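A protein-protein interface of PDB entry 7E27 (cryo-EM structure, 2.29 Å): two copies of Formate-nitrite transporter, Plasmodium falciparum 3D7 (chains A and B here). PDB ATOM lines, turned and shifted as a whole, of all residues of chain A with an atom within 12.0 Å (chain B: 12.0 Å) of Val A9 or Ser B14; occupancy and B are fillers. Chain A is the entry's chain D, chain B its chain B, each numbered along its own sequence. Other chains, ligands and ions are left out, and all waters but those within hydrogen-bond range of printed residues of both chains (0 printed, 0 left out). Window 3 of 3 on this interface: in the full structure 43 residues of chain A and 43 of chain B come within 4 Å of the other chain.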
ATOM      1  N   LYS A   7      -8.153  17.715  -4.842  1.00  0.00           N
ATOM      2  CA  LYS A   7      -9.110  16.662  -5.160  1.00  0.00           C
ATOM      3  C   LYS A   7      -8.508  15.287  -4.896  1.00  0.00           C
ATOM      4  O   LYS A   7      -7.526  14.895  -5.525  1.00  0.00           O
ATOM      5  CB  LYS A   7      -9.566  16.769  -6.616  1.00  0.00           C
ATOM      6  N   TYR A   8      -9.105  14.557  -3.962  1.00  0.00           N
ATOM      7  CA  TYR A   8      -8.611  13.256  -3.542  1.00  0.00           C
ATOM      8  C   TYR A   8      -9.545  12.162  -4.042  1.00  0.00           C
ATOM      9  O   TYR A   8     -10.764  12.347  -4.086  1.00  0.00           O
ATOM     10  CB  TYR A   8      -8.486  13.184  -2.018  1.00  0.00           C
ATOM     11  CG  TYR A   8      -7.782  14.374  -1.404  1.00  0.00           C
ATOM     12  CD1 TYR A   8      -6.396  14.450  -1.388  1.00  0.00           C
ATOM     13  CD2 TYR A   8      -8.504  15.420  -0.839  1.00  0.00           C
ATOM     14  CE1 TYR A   8      -5.748  15.535  -0.830  1.00  0.00           C
ATOM     15  CE2 TYR A   8      -7.864  16.510  -0.279  1.00  0.00           C
ATOM     16  CZ  TYR A   8      -6.488  16.560  -0.277  1.00  0.00           C
ATOM     17  OH  TYR A   8      -5.847  17.641   0.280  1.00  0.00           O
ATOM     18  N   VAL A   9      -8.964  11.031  -4.426  1.00  0.00           N
ATOM     19  CA  VAL A   9      -9.712   9.866  -4.884  1.00  0.00           C
ATOM     20  C   VAL A   9      -9.685   8.830  -3.771  1.00  0.00           C
ATOM     21  O   VAL A   9      -8.612   8.368  -3.365  1.00  0.00           O
ATOM     22  CB  VAL A   9      -9.135   9.298  -6.191  1.00  0.00           C
ATOM     23  CG1 VAL A   9      -9.708   7.920  -6.476  1.00  0.00           C
ATOM     24  CG2 VAL A   9      -9.421  10.240  -7.346  1.00  0.00           C
ATOM     25  N   LEU A  10     -10.864   8.474  -3.267  1.00  0.00           N
ATOM     26  CA  LEU A  10     -10.973   7.457  -2.231  1.00  0.00           C
ATOM     27  C   LEU A  10     -11.454   6.124  -2.780  1.00  0.00           C
ATOM     28  O   LEU A  10     -10.925   5.074  -2.405  1.00  0.00           O
ATOM     29  CB  LEU A  10     -11.924   7.918  -1.124  1.00  0.00           C
ATOM     30  CG  LEU A  10     -11.312   8.659   0.062  1.00  0.00           C
ATOM     31  CD1 LEU A  10     -10.896  10.065  -0.320  1.00  0.00           C
ATOM     32  CD2 LEU A  10     -12.284   8.675   1.222  1.00  0.00           C
ATOM     33  N   ASP A  11     -12.449   6.152  -3.658  1.00  0.00           N
ATOM     34  CA  ASP A  11     -13.015   4.941  -4.246  1.00  0.00           C
ATOM     35  C   ASP A  11     -12.834   5.049  -5.751  1.00  0.00           C
ATOM     36  O   ASP A  11     -13.625   5.747  -6.420  1.00  0.00           O
ATOM     37  CB  ASP A  11     -14.485   4.788  -3.863  1.00  0.00           C
ATOM     38  CG  ASP A  11     -14.990   3.360  -4.006  1.00  0.00           C
ATOM     39  OD1 ASP A  11     -14.629   2.667  -4.981  1.00  0.00           O
ATOM     40  OD2 ASP A  11     -15.764   2.928  -3.127  1.00  0.00           O
ATOM     41  N   PRO A  12     -11.829   4.394  -6.323  1.00  0.00           N
ATOM     42  CA  PRO A  12     -11.633   4.460  -7.772  1.00  0.00           C
ATOM     43  C   PRO A  12     -12.620   3.584  -8.530  1.00  0.00           C
ATOM     44  O   PRO A  12     -13.464   2.897  -7.954  1.00  0.00           O
ATOM     45  CB  PRO A  12     -10.200   3.958  -7.955  1.00  0.00           C
ATOM     46  CG  PRO A  12      -9.600   3.892  -6.592  1.00  0.00           C
ATOM     47  CD  PRO A  12     -10.722   3.700  -5.651  1.00  0.00           C
ATOM     48  N   VAL A  13     -12.493   3.615  -9.859  1.00  0.00           N
ATOM     49  CA  VAL A  13     -13.415   2.886 -10.722  1.00  0.00           C
ATOM     50  C   VAL A  13     -13.068   1.406 -10.711  1.00  0.00           C
ATOM     51  O   VAL A  13     -11.923   1.014 -10.959  1.00  0.00           O
ATOM     52  CB  VAL A  13     -13.379   3.464 -12.145  1.00  0.00           C
ATOM     53  CG1 VAL A  13     -14.296   2.687 -13.068  1.00  0.00           C
ATOM     54  CG2 VAL A  13     -13.760   4.925 -12.127  1.00  0.00           C
ATOM     55  N   SER A  14     -14.063   0.572 -10.435  1.00  0.00           N
ATOM     56  CA  SER A  14     -13.858  -0.864 -10.332  1.00  0.00           C
ATOM     57  C   SER A  14     -13.789  -1.490 -11.722  1.00  0.00           C
ATOM     58  O   SER A  14     -14.701  -1.317 -12.535  1.00  0.00           O
ATOM     59  CB  SER A  14     -14.983  -1.485  -9.508  1.00  0.00           C
ATOM     60  OG  SER A  14     -14.802  -2.872  -9.335  1.00  0.00           O
ATOM     61  N   ILE A  15     -12.699  -2.208 -11.997  1.00  0.00           N
ATOM     62  CA  ILE A  15     -12.485  -2.869 -13.277  1.00  0.00           C
ATOM     63  C   ILE A  15     -12.330  -4.366 -13.058  1.00  0.00           C
ATOM     64  O   ILE A  15     -12.233  -4.854 -11.930  1.00  0.00           O
ATOM     65  CB  ILE A  15     -11.233  -2.376 -14.017  1.00  0.00           C
ATOM     66  CG1 ILE A  15     -10.034  -2.728 -13.144  1.00  0.00           C
ATOM     67  CG2 ILE A  15     -11.335  -0.895 -14.318  1.00  0.00           C
ATOM     68  CD1 ILE A  15      -8.832  -3.052 -13.840  1.00  0.00           C
ATOM     69  N   LYS A  16     -12.296  -5.090 -14.170  1.00  0.00           N
ATOM     70  CA  LYS A  16     -11.894  -6.484 -14.196  1.00  0.00           C
ATOM     71  C   LYS A  16     -11.241  -6.786 -15.535  1.00  0.00           C
ATOM     72  O   LYS A  16     -11.597  -6.208 -16.561  1.00  0.00           O
ATOM     73  CB  LYS A  16     -13.076  -7.430 -13.956  1.00  0.00           C
ATOM     74  CG  LYS A  16     -14.165  -7.400 -14.994  1.00  0.00           C
ATOM     75  CD  LYS A  16     -15.097  -8.556 -14.789  1.00  0.00           C
ATOM     76  CE  LYS A  16     -16.076  -8.679 -15.915  1.00  0.00           C
ATOM     77  NZ  LYS A  16     -16.463 -10.099 -16.082  1.00  0.00           N
ATOM     78  N   VAL B   9      -0.416  13.336 -20.635  1.00  0.00           N
ATOM     79  CA  VAL B   9      -1.231  12.848 -19.530  1.00  0.00           C
ATOM     80  C   VAL B   9      -0.372  12.866 -18.275  1.00  0.00           C
ATOM     81  O   VAL B   9       0.668  12.198 -18.213  1.00  0.00           O
ATOM     82  CB  VAL B   9      -1.781  11.440 -19.809  1.00  0.00           C
ATOM     83  CG1 VAL B   9      -2.346  10.822 -18.539  1.00  0.00           C
ATOM     84  CG2 VAL B   9      -2.846  11.496 -20.890  1.00  0.00           C
ATOM     85  N   LEU B  10      -0.795  13.642 -17.281  1.00  0.00           N
ATOM     86  CA  LEU B  10      -0.084  13.708 -16.011  1.00  0.00           C
ATOM     87  C   LEU B  10      -0.780  12.914 -14.920  1.00  0.00           C
ATOM     88  O   LEU B  10      -0.120  12.210 -14.150  1.00  0.00           O
ATOM     89  CB  LEU B  10       0.068  15.161 -15.557  1.00  0.00           C
ATOM     90  CG  LEU B  10       1.335  15.899 -15.983  1.00  0.00           C
ATOM     91  CD1 LEU B  10       1.302  16.247 -17.458  1.00  0.00           C
ATOM     92  CD2 LEU B  10       1.523  17.139 -15.136  1.00  0.00           C
ATOM     93  N   ASP B  11      -2.100  13.018 -14.838  1.00  0.00           N
ATOM     94  CA  ASP B  11      -2.886  12.323 -13.825  1.00  0.00           C
ATOM     95  C   ASP B  11      -3.869  11.423 -14.558  1.00  0.00           C
ATOM     96  O   ASP B  11      -4.914  11.912 -15.037  1.00  0.00           O
ATOM     97  CB  ASP B  11      -3.602  13.317 -12.914  1.00  0.00           C
ATOM     98  CG  ASP B  11      -4.014  12.712 -11.580  1.00  0.00           C
ATOM     99  OD1 ASP B  11      -4.466  11.548 -11.539  1.00  0.00           O
ATOM    100  OD2 ASP B  11      -3.887  13.418 -10.560  1.00  0.00           O
ATOM    101  N   PRO B  12      -3.588  10.131 -14.676  1.00  0.00           N
ATOM    102  CA  PRO B  12      -4.517   9.231 -15.362  1.00  0.00           C
ATOM    103  C   PRO B  12      -5.722   8.879 -14.500  1.00  0.00           C
ATOM    104  O   PRO B  12      -5.856   9.309 -13.354  1.00  0.00           O
ATOM    105  CB  PRO B  12      -3.664   7.995 -15.645  1.00  0.00           C
ATOM    106  CG  PRO B  12      -2.256   8.374 -15.339  1.00  0.00           C
ATOM    107  CD  PRO B  12      -2.325   9.459 -14.338  1.00  0.00           C
ATOM    108  N   VAL B  13      -6.611   8.068 -15.081  1.00  0.00           N
ATOM    109  CA  VAL B  13      -7.852   7.703 -14.408  1.00  0.00           C
ATOM    110  C   VAL B  13      -7.570   6.653 -13.345  1.00  0.00           C
ATOM    111  O   VAL B  13      -6.963   5.613 -13.618  1.00  0.00           O
ATOM    112  CB  VAL B  13      -8.884   7.208 -15.433  1.00  0.00           C
ATOM    113  CG1 VAL B  13     -10.165   6.777 -14.746  1.00  0.00           C
ATOM    114  CG2 VAL B  13      -9.167   8.284 -16.454  1.00  0.00           C
ATOM    115  N   SER B  14      -8.024   6.917 -12.127  1.00  0.00           N
ATOM    116  CA  SER B  14      -7.772   6.027 -11.004  1.00  0.00           C
ATOM    117  C   SER B  14      -8.729   4.839 -11.046  1.00  0.00           C
ATOM    118  O   SER B  14      -9.948   5.016 -11.095  1.00  0.00           O
ATOM    119  CB  SER B  14      -7.920   6.801  -9.695  1.00  0.00           C
ATOM    120  OG  SER B  14      -7.634   5.994  -8.574  1.00  0.00           O
ATOM    121  N   ILE B  15      -8.171   3.627 -11.038  1.00  0.00           N
ATOM    122  CA  ILE B  15      -8.946   2.395 -11.072  1.00  0.00           C
ATOM    123  C   ILE B  15      -8.643   1.567  -9.833  1.00  0.00           C
ATOM    124  O   ILE B  15      -7.738   1.868  -9.051  1.00  0.00           O
ATOM    125  CB  ILE B  15      -8.649   1.523 -12.299  1.00  0.00           C
ATOM    126  CG1 ILE B  15      -7.186   1.106 -12.205  1.00  0.00           C
ATOM    127  CG2 ILE B  15      -8.977   2.263 -13.579  1.00  0.00           C
ATOM    128  CD1 ILE B  15      -6.870  -0.183 -12.726  1.00  0.00           C
ATOM    129  N   LYS B  16      -9.415   0.500  -9.675  1.00  0.00           N
ATOM    130  CA  LYS B  16      -9.126  -0.556  -8.721  1.00  0.00           C
ATOM    131  C   LYS B  16      -9.656  -1.872  -9.262  1.00  0.00           C
ATOM    132  O   LYS B  16     -10.664  -1.911  -9.966  1.00  0.00           O
ATOM    133  CB  LYS B  16      -9.731  -0.266  -7.341  1.00  0.00           C
ATOM    134  CG  LYS B  16     -11.234  -0.196  -7.283  1.00  0.00           C
ATOM    135  CD  LYS B  16     -11.687  -0.195  -5.854  1.00  0.00           C
ATOM    136  CE  LYS B  16     -13.176  -0.327  -5.750  1.00  0.00           C
ATOM    137  NZ  LYS B  16     -13.524  -1.010  -4.485  1.00  0.00           N
ATOM    138  N   SER B  17      -8.963  -2.953  -8.941  1.00  0.00           N
ATOM    139  CA  SER B  17      -9.396  -4.283  -9.331  1.00  0.00           C
ATOM    140  C   SER B  17      -9.725  -5.165  -8.139  1.00  0.00           C
ATOM    141  O   SER B  17      -9.835  -6.384  -8.299  1.00  0.00           O
ATOM    142  CB  SER B  17      -8.326  -4.965 -10.186  1.00  0.00           C
ATOM    143  OG  SER B  17      -8.731  -6.273 -10.525  1.00  0.00           O
ATOM    144  N   VAL B  18      -9.873  -4.586  -6.951  1.00  0.00           N
ATOM    145  CA  VAL B  18     -10.151  -5.313  -5.723  1.00  0.00           C
ATOM    146  C   VAL B  18     -11.484  -4.823  -5.171  1.00  0.00           C
ATOM    147  O   VAL B  18     -12.030  -3.814  -5.613  1.00  0.00           O
ATOM    148  CB  VAL B  18      -9.021  -5.133  -4.689  1.00  0.00           C
ATOM    149  CG1 VAL B  18      -7.689  -5.561  -5.288  1.00  0.00           C
ATOM    150  CG2 VAL B  18      -8.954  -3.691  -4.239  1.00  0.00           C
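The backbone carbonyl oxygen of Lys B16 is in hydrogen-bond range of the backbone NH of Ile A15 (2.9 Å).
The side-chain carboxylate (OD1) of Asp A11 is in salt-bridge range of the side-chain amino group (NZ) of Lys B16 (3.9 Å).
O of Val A13 sits at hydrogen-bond distance from N of Lys B16 (2.9 Å).
O of Ser B14 is in hydrogen-bond range of N of Val A13 (3.2 Å).
The side-chain amino group (NZ) of Lys B16 is in hydrogen-bond range of the backbone carbonyl oxygen (O) of Val B18, at 3.4 Å.
Among the printed residues, pairs that only touch across the chains: Val A13 with Ile B15 (3.3 Å), Pro A12 with Ser B14 (3.3 Å), Ser A14 with Lys B16 (3.4 Å), Pro A12 with Ile B15 (3.4 Å), Val A9 with Ser B14 (3.5 Å), Ile A15 with Ile B15 (3.6 Å), Pro A12 with Lys B16 (3.9 Å) and Ile A15 with Ser B17 (3.9 Å).
Printed residues of chain B within 4 Å of Val A9: Ser B14.
Of chain A, only Val A9, Pro A12 and Val A13 come within 4 Å of Ser B14.
No residue of chain B comes within 4 Å of Lys A7.
No residue of chain B comes within 4 Å of Leu A10.
Val A13 touches just these residues of chain B: Ser B14 (3.2 Å), Ile B15 (3.3 Å) and Lys B16 (2.9 Å).
No residue of chain A comes within 4 Å of Val B13.
Of chain A, only Pro A12 (3.4 Å), Val A13 (3.3 Å) and Ile A15 (3.6 Å) come within 4 Å of Ile B15.
Of the printed residues of chain A, Ser B17 touches Ile A15.
Printed residues of chain B within 4 Å of Asp A11: Lys B16.
Of the printed residues of chain B, Ser A14 touches Lys B16.
Of the printed residues of chain A, Lys B16 touches Asp A11 (3.4 Å), Pro A12 (3.9 Å), Val A13 (2.9 Å), Ser A14 (3.4 Å) and Ile A15 (2.9 Å).
Of the printed residues of chain B, Ile A15 touches Ile B15, Lys B16 and Ser B17.
Leu B10 touches none of the printed residues of chain A.
The nearest residue of chain B that does not touch Val A9 is Ile B15 (6.5 Å).
The nearest printed residue of chain B that does not touch Asp A11 is Ser B14 (6.0 Å).
Of the 10 printed residues of chain A, 6 touch a printed residue of chain B.
Hydrophobic or aromatic side chains of chain A that line the printed part of chain B: Val A9, Pro A12, Val A13 and Ile A15.
Among the printed residues, Asp or Glu carboxylates within 4 Å of a Lys or Arg side-chain nitrogen of the other chain: Asp A11 with Lys B16 (3.9 Å).
Val A13 touches Ser B14, but with the chains exchanged Ser A14 does not touch Val B13 (8.5 Å).
Val A13 touches Lys B16, but with the chains exchanged Lys A16 does not touch Val B13 (12.0 Å).
Ile A15 touches its own counterpart, Ile B15.
Ile A15 touches Lys B16, but with the chains exchanged Lys A16 does not touch Ile B15 (7.5 Å).
Of the 12 pairs that touch across the chains among the printed residues, 1 has its exchanged pair printed and touching as well.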
